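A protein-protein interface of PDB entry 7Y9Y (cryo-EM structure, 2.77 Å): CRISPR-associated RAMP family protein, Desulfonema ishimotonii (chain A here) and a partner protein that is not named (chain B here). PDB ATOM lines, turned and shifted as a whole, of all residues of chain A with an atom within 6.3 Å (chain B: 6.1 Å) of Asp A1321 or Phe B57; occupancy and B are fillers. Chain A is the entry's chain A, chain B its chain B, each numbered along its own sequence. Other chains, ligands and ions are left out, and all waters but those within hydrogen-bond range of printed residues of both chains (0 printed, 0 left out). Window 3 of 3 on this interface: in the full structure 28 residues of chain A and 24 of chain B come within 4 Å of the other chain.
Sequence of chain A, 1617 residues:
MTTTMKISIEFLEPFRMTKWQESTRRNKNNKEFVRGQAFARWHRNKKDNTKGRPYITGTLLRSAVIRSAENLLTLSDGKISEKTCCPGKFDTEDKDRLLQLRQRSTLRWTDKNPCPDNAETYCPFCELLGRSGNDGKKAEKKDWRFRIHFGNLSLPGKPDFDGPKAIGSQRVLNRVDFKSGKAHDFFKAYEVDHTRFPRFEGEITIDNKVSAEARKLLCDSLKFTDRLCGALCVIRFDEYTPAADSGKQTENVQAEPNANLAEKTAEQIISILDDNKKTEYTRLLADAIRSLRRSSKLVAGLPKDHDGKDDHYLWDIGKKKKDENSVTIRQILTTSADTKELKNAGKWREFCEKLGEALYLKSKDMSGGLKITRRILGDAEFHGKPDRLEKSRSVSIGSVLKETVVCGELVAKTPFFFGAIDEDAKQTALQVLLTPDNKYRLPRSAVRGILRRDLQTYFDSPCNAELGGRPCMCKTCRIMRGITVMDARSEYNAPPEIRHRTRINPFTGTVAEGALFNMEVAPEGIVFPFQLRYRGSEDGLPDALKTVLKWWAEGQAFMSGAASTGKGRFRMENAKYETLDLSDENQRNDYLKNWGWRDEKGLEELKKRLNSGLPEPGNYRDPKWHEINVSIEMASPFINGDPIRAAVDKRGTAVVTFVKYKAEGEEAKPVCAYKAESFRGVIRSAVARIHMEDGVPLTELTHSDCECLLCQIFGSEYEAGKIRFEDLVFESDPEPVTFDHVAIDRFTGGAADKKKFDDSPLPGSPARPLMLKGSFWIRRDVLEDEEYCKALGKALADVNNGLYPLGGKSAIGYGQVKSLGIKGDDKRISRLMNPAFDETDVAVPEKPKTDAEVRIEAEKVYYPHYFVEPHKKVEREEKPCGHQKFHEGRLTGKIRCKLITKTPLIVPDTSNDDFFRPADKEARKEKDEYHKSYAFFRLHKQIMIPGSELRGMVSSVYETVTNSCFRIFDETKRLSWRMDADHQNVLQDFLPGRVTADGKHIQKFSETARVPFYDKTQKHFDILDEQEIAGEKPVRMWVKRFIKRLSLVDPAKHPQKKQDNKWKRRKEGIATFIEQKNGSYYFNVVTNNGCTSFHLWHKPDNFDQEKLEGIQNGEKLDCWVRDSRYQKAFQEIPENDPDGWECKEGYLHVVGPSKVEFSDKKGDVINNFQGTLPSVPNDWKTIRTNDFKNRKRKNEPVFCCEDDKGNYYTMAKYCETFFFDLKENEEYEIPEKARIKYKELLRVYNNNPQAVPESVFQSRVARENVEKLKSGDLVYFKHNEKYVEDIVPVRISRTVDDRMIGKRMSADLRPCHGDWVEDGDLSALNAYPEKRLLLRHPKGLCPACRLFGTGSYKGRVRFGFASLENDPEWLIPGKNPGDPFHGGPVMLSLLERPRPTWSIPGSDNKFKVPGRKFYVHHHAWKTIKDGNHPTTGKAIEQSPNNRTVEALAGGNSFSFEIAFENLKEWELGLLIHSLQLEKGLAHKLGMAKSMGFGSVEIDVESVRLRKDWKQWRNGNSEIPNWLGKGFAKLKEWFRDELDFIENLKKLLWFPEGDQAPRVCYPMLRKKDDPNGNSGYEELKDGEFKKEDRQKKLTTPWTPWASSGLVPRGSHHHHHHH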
ATOM      1  N   TRP A1316      24.363  -1.968 -19.574  1.00  0.00           N
ATOM      2  CA  TRP A1316      23.356  -1.909 -18.515  1.00  0.00           C
ATOM      3  C   TRP A1316      23.126  -0.450 -18.141  1.00  0.00           C
ATOM      4  O   TRP A1316      23.945   0.163 -17.453  1.00  0.00           O
ATOM      5  CB  TRP A1316      23.801  -2.728 -17.310  1.00  0.00           C
ATOM      6  CG  TRP A1316      22.682  -3.143 -16.408  1.00  0.00           C
ATOM      7  CD1 TRP A1316      22.540  -2.831 -15.090  1.00  0.00           C
ATOM      8  CD2 TRP A1316      21.551  -3.957 -16.751  1.00  0.00           C
ATOM      9  NE1 TRP A1316      21.391  -3.392 -14.590  1.00  0.00           N
ATOM     10  CE2 TRP A1316      20.767  -4.089 -15.589  1.00  0.00           C
ATOM     11  CE3 TRP A1316      21.127  -4.582 -17.927  1.00  0.00           C
ATOM     12  CZ2 TRP A1316      19.582  -4.821 -15.568  1.00  0.00           C
ATOM     13  CZ3 TRP A1316      19.951  -5.308 -17.903  1.00  0.00           C
ATOM     14  CH2 TRP A1316      19.193  -5.421 -16.732  1.00  0.00           C
ATOM     15  N   GLU A1318      20.213   0.424 -16.584  1.00  0.00           N
ATOM     16  CA  GLU A1318      19.249   0.400 -15.493  1.00  0.00           C
ATOM     17  C   GLU A1318      19.978   0.495 -14.152  1.00  0.00           C
ATOM     18  O   GLU A1318      21.210   0.499 -14.081  1.00  0.00           O
ATOM     19  CB  GLU A1318      18.384  -0.851 -15.601  1.00  0.00           C
ATOM     20  CG  GLU A1318      17.510  -0.867 -16.840  1.00  0.00           C
ATOM     21  CD  GLU A1318      16.721  -2.147 -16.982  1.00  0.00           C
ATOM     22  OE1 GLU A1318      16.791  -2.992 -16.064  1.00  0.00           O
ATOM     23  OE2 GLU A1318      16.029  -2.308 -18.009  1.00  0.00           O
ATOM     24  N   ASP A1319      19.211   0.578 -13.065  1.00  0.00           N
ATOM     25  CA  ASP A1319      19.786   0.696 -11.732  1.00  0.00           C
ATOM     26  C   ASP A1319      19.983  -0.677 -11.103  1.00  0.00           C
ATOM     27  O   ASP A1319      19.288  -1.037 -10.149  1.00  0.00           O
ATOM     28  CB  ASP A1319      18.902   1.569 -10.840  1.00  0.00           C
ATOM     29  CG  ASP A1319      19.659   2.162  -9.664  1.00  0.00           C
ATOM     30  OD1 ASP A1319      20.382   1.411  -8.975  1.00  0.00           O
ATOM     31  OD2 ASP A1319      19.532   3.382  -9.430  1.00  0.00           O
ATOM     32  N   GLY A1320      20.923  -1.448 -11.637  1.00  0.00           N
ATOM     33  CA  GLY A1320      21.252  -2.742 -11.073  1.00  0.00           C
ATOM     34  C   GLY A1320      22.725  -3.020 -11.243  1.00  0.00           C
ATOM     35  O   GLY A1320      23.350  -2.561 -12.204  1.00  0.00           O
ATOM     36  N   ASP A1321      23.286  -3.767 -10.296  1.00  0.00           N
ATOM     37  CA  ASP A1321      24.710  -4.071 -10.345  1.00  0.00           C
ATOM     38  C   ASP A1321      25.037  -4.941 -11.552  1.00  0.00           C
ATOM     39  O   ASP A1321      25.987  -4.655 -12.289  1.00  0.00           O
ATOM     40  CB  ASP A1321      25.161  -4.749  -9.046  1.00  0.00           C
ATOM     41  CG  ASP A1321      24.438  -6.058  -8.782  1.00  0.00           C
ATOM     42  OD1 ASP A1321      23.303  -6.223  -9.275  1.00  0.00           O
ATOM     43  OD2 ASP A1321      25.006  -6.924  -8.082  1.00  0.00           O
ATOM     44  N   LEU A1322      24.259  -6.002 -11.757  1.00  0.00           N
ATOM     45  CA  LEU A1322      24.393  -7.014 -12.796  1.00  0.00           C
ATOM     46  C   LEU A1322      25.656  -7.848 -12.592  1.00  0.00           C
ATOM     47  O   LEU A1322      25.868  -8.805 -13.334  1.00  0.00           O
ATOM     48  CB  LEU A1322      24.391  -6.431 -14.225  1.00  0.00           C
ATOM     49  CG  LEU A1322      23.974  -7.359 -15.370  1.00  0.00           C
ATOM     50  CD1 LEU A1322      22.492  -7.673 -15.289  1.00  0.00           C
ATOM     51  CD2 LEU A1322      24.320  -6.747 -16.718  1.00  0.00           C
ATOM     52  N   SER A1323      26.497  -7.528 -11.608  1.00  0.00           N
ATOM     53  CA  SER A1323      27.666  -8.342 -11.312  1.00  0.00           C
ATOM     54  C   SER A1323      27.342  -9.502 -10.385  1.00  0.00           C
ATOM     55  O   SER A1323      28.184 -10.388 -10.206  1.00  0.00           O
ATOM     56  CB  SER A1323      28.768  -7.479 -10.694  1.00  0.00           C
ATOM     57  OG  SER A1323      29.082  -6.384 -11.537  1.00  0.00           O
ATOM     58  N   ALA A1324      26.150  -9.510  -9.786  1.00  0.00           N
ATOM     59  CA  ALA A1324      25.722 -10.667  -9.011  1.00  0.00           C
ATOM     60  C   ALA A1324      25.523 -11.883  -9.901  1.00  0.00           C
ATOM     61  O   ALA A1324      25.830 -13.009  -9.491  1.00  0.00           O
ATOM     62  CB  ALA A1324      24.436 -10.347  -8.250  1.00  0.00           C
ATOM     63  N   LEU A1325      25.017 -11.682 -11.114  1.00  0.00           N
ATOM     64  CA  LEU A1325      24.819 -12.762 -12.069  1.00  0.00           C
ATOM     65  C   LEU A1325      26.064 -13.058 -12.894  1.00  0.00           C
ATOM     66  O   LEU A1325      25.965 -13.740 -13.919  1.00  0.00           O
ATOM     67  CB  LEU A1325      23.628 -12.467 -12.992  1.00  0.00           C
ATOM     68  CG  LEU A1325      22.182 -12.445 -12.463  1.00  0.00           C
ATOM     69  CD1 LEU A1325      21.982 -11.675 -11.164  1.00  0.00           C
ATOM     70  CD2 LEU A1325      21.241 -11.919 -13.535  1.00  0.00           C
ATOM     71  N   LEU A1334      20.470 -10.334 -20.745  1.00  0.00           N
ATOM     72  CA  LEU A1334      20.034  -9.064 -20.184  1.00  0.00           C
ATOM     73  C   LEU A1334      20.617  -7.865 -20.919  1.00  0.00           C
ATOM     74  O   LEU A1334      20.209  -6.733 -20.641  1.00  0.00           O
ATOM     75  CB  LEU A1334      20.403  -8.993 -18.702  1.00  0.00           C
ATOM     76  CG  LEU A1334      19.486  -9.800 -17.782  1.00  0.00           C
ATOM     77  CD1 LEU A1334      20.266 -10.360 -16.613  1.00  0.00           C
ATOM     78  CD2 LEU A1334      18.327  -8.951 -17.297  1.00  0.00           C
ATOM     79  N   ASN B  52      11.394  -6.909 -20.747  1.00  0.00           N
ATOM     80  CA  ASN B  52      11.202  -6.469 -19.366  1.00  0.00           C
ATOM     81  C   ASN B  52      12.456  -6.746 -18.535  1.00  0.00           C
ATOM     82  O   ASN B  52      12.455  -7.552 -17.603  1.00  0.00           O
ATOM     83  CB  ASN B  52       9.962  -7.127 -18.749  1.00  0.00           C
ATOM     84  CG  ASN B  52       9.100  -6.147 -17.979  1.00  0.00           C
ATOM     85  OD1 ASN B  52       9.534  -5.044 -17.652  1.00  0.00           O
ATOM     86  ND2 ASN B  52       7.867  -6.545 -17.690  1.00  0.00           N
ATOM     87  N   ARG B  53      13.539  -6.063 -18.908  1.00  0.00           N
ATOM     88  CA  ARG B  53      14.832  -6.304 -18.273  1.00  0.00           C
ATOM     89  C   ARG B  53      14.832  -6.136 -16.755  1.00  0.00           C
ATOM     90  O   ARG B  53      15.461  -6.968 -16.080  1.00  0.00           O
ATOM     91  CB  ARG B  53      15.904  -5.403 -18.902  1.00  0.00           C
ATOM     92  CG  ARG B  53      16.048  -5.530 -20.407  1.00  0.00           C
ATOM     93  CD  ARG B  53      17.294  -4.804 -20.891  1.00  0.00           C
ATOM     94  NE  ARG B  53      17.255  -4.531 -22.323  1.00  0.00           N
ATOM     95  CZ  ARG B  53      17.661  -5.381 -23.256  1.00  0.00           C
ATOM     96  NH1 ARG B  53      18.138  -6.574 -22.945  1.00  0.00           N
ATOM     97  NH2 ARG B  53      17.583  -5.025 -24.535  1.00  0.00           N
ATOM     98  N   PRO B  54      14.208  -5.111 -16.159  1.00  0.00           N
ATOM     99  CA  PRO B  54      14.241  -5.028 -14.685  1.00  0.00           C
ATOM    100  C   PRO B  54      13.595  -6.221 -14.001  1.00  0.00           C
ATOM    101  O   PRO B  54      14.178  -6.795 -13.071  1.00  0.00           O
ATOM    102  CB  PRO B  54      13.488  -3.721 -14.395  1.00  0.00           C
ATOM    103  CG  PRO B  54      13.598  -2.933 -15.642  1.00  0.00           C
ATOM    104  CD  PRO B  54      13.547  -3.934 -16.747  1.00  0.00           C
ATOM    105  N   ASN B  55      12.397  -6.614 -14.440  1.00  0.00           N
ATOM    106  CA  ASN B  55      11.707  -7.735 -13.811  1.00  0.00           C
ATOM    107  C   ASN B  55      12.449  -9.045 -14.044  1.00  0.00           C
ATOM    108  O   ASN B  55      12.561  -9.873 -13.131  1.00  0.00           O
ATOM    109  CB  ASN B  55      10.274  -7.821 -14.337  1.00  0.00           C
ATOM    110  CG  ASN B  55       9.434  -8.828 -13.579  1.00  0.00           C
ATOM    111  OD1 ASN B  55       8.454  -9.355 -14.106  1.00  0.00           O
ATOM    112  ND2 ASN B  55       9.807  -9.096 -12.333  1.00  0.00           N
ATOM    113  N   SER B  56      12.960  -9.253 -15.262  1.00  0.00           N
ATOM    114  CA  SER B  56      13.717 -10.467 -15.549  1.00  0.00           C
ATOM    115  C   SER B  56      14.984 -10.534 -14.707  1.00  0.00           C
ATOM    116  O   SER B  56      15.336 -11.598 -14.184  1.00  0.00           O
ATOM    117  CB  SER B  56      14.052 -10.532 -17.038  1.00  0.00           C
ATOM    118  OG  SER B  56      12.875 -10.627 -17.821  1.00  0.00           O
ATOM    119  N   PHE B  57      15.677  -9.403 -14.560  1.00  0.00           N
ATOM    120  CA  PHE B  57      16.855  -9.353 -13.703  1.00  0.00           C
ATOM    121  C   PHE B  57      16.502  -9.659 -12.256  1.00  0.00           C
ATOM    122  O   PHE B  57      17.225 -10.394 -11.576  1.00  0.00           O
ATOM    123  CB  PHE B  57      17.522  -7.985 -13.810  1.00  0.00           C
ATOM    124  CG  PHE B  57      18.675  -7.800 -12.869  1.00  0.00           C
ATOM    125  CD1 PHE B  57      19.751  -8.671 -12.887  1.00  0.00           C
ATOM    126  CD2 PHE B  57      18.682  -6.754 -11.964  1.00  0.00           C
ATOM    127  CE1 PHE B  57      20.810  -8.500 -12.018  1.00  0.00           C
ATOM    128  CE2 PHE B  57      19.739  -6.579 -11.094  1.00  0.00           C
ATOM    129  CZ  PHE B  57      20.804  -7.453 -11.122  1.00  0.00           C
ATOM    130  N   SER B  58      15.398  -9.095 -11.762  1.00  0.00           N
ATOM    131  CA  SER B  58      14.995  -9.349 -10.383  1.00  0.00           C
ATOM    132  C   SER B  58      14.699 -10.827 -10.163  1.00  0.00           C
ATOM    133  O   SER B  58      15.141 -11.421  -9.173  1.00  0.00           O
ATOM    134  CB  SER B  58      13.779  -8.492 -10.029  1.00  0.00           C
ATOM    135  OG  SER B  58      14.004  -7.133 -10.362  1.00  0.00           O
ATOM    136  N   GLN B  59      13.959 -11.443 -11.091  1.00  0.00           N
ATOM    137  CA  GLN B  59      13.634 -12.859 -10.951  1.00  0.00           C
ATOM    138  C   GLN B  59      14.880 -13.733 -11.040  1.00  0.00           C
ATOM    139  O   GLN B  59      15.028 -14.687 -10.268  1.00  0.00           O
ATOM    140  CB  GLN B  59      12.608 -13.272 -12.004  1.00  0.00           C
ATOM    141  CG  GLN B  59      11.270 -12.569 -11.857  1.00  0.00           C
ATOM    142  CD  GLN B  59      10.463 -12.569 -13.136  1.00  0.00           C
ATOM    143  OE1 GLN B  59       9.451 -11.879 -13.242  1.00  0.00           O
ATOM    144  NE2 GLN B  59      10.905 -13.346 -14.115  1.00  0.00           N
ATOM    145  N   LEU B  60      15.793 -13.423 -11.966  1.00  0.00           N
ATOM    146  CA  LEU B  60      17.018 -14.210 -12.080  1.00  0.00           C
ATOM    147  C   LEU B  60      17.882 -14.076 -10.832  1.00  0.00           C
ATOM    148  O   LEU B  60      18.451 -15.063 -10.352  1.00  0.00           O
ATOM    149  CB  LEU B  60      17.795 -13.789 -13.327  1.00  0.00           C
ATOM    150  CG  LEU B  60      17.192 -14.235 -14.662  1.00  0.00           C
ATOM    151  CD1 LEU B  60      17.808 -13.469 -15.823  1.00  0.00           C
ATOM    152  CD2 LEU B  60      17.353 -15.736 -14.858  1.00  0.00           C
ATOM    153  N   SER B  61      17.989 -12.860 -10.288  1.00  0.00           N
ATOM    154  CA  SER B  61      18.766 -12.657  -9.070  1.00  0.00           C
ATOM    155  C   SER B  61      18.143 -13.385  -7.888  1.00  0.00           C
ATOM    156  O   SER B  61      18.860 -13.949  -7.053  1.00  0.00           O
ATOM    157  CB  SER B  61      18.897 -11.163  -8.777  1.00  0.00           C
ATOM    158  OG  SER B  61      19.672 -10.938  -7.613  1.00  0.00           O
ATOM    159  N   GLN B  62      16.811 -13.377  -7.790  1.00  0.00           N
ATOM    160  CA  GLN B  62      16.147 -14.133  -6.733  1.00  0.00           C
ATOM    161  C   GLN B  62      16.395 -15.629  -6.891  1.00  0.00           C
ATOM    162  O   GLN B  62      16.605 -16.340  -5.901  1.00  0.00           O
ATOM    163  CB  GLN B  62      14.649 -13.835  -6.733  1.00  0.00           C
ATOM    164  CG  GLN B  62      14.219 -12.764  -5.749  1.00  0.00           C
ATOM    165  CD  GLN B  62      12.887 -12.146  -6.118  1.00  0.00           C
ATOM    166  OE1 GLN B  62      12.175 -12.653  -6.984  1.00  0.00           O
ATOM    167  NE2 GLN B  62      12.543 -11.044  -5.463  1.00  0.00           N
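Of chain B, only Phe B57 comes within 4 Å of Asp A1321.
Phe B57 touches just these residues of chain A: Asp A1321 (3.3 Å), Leu A1322 (3.8 Å), Leu A1325 (3.5 Å) and Leu A1334 (3.7 Å).
Of the printed residues of chain B, Leu A1325 touches Phe B57 (3.5 Å), Leu B60 (3.9 Å) and Ser B61 (3.9 Å).
Of the printed residues of chain B, Trp A1316 touches Arg B53.
Of the printed residues of chain A, Ser B61 touches Leu A1325 (3.9 Å).
Ala A1324 touches none of the printed residues of chain B.
The nearest printed residue of chain A that does not touch Phe B57 is Trp A1316 (4.1 Å).
NE1 of Trp A1316 lies close to O of Gly A1320 (3.2 Å).
The side-chain carboxylate of Asp A1321 sits at hydrogen-bond distance from the backbone NH of Ala A1324, 3.3 Å away.
The backbone carbonyl oxygen (O) of Pro B54 sits at hydrogen-bond distance from the side-chain hydroxyl (OG) of Ser B58, 2.7 Å away.
NH1 of Arg B53 sits at hydrogen-bond distance from O of Leu A1334, 3.1 Å away.
The side-chain carboxylate (OE1) of Glu A1318 lies close to the backbone nitrogen (N) of Pro B54 (3.3 Å).
Among the printed residues, pairs that only touch across the chains: Glu A1318 with Arg B53 (3.2 Å), Asp A1321 with Phe B57 (3.3 Å), Leu A1325 with Phe B57 (3.5 Å), Leu A1334 with Phe B57 (3.7 Å), Leu A1322 with Phe B57 (3.8 Å), Leu A1325 with Leu B60 (3.9 Å), Leu A1325 with Ser B61 (3.9 Å) and Trp A1316 with Arg B53 (3.9 Å).
Printed residues of chain A that touch a printed residue of chain B: Trp A1316, Glu A1318, Asp A1321, Leu A1322, Leu A1325 and Leu A1334.
Hydrophobic or aromatic side chains of chain A that line the printed part of chain B: Trp A1316, Leu A1322, Leu A1325 and Leu A1334.
Printed residues of chain B that touch a printed residue of chain A: Arg B53, Pro B54, Phe B57, Leu B60 and Ser B61.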
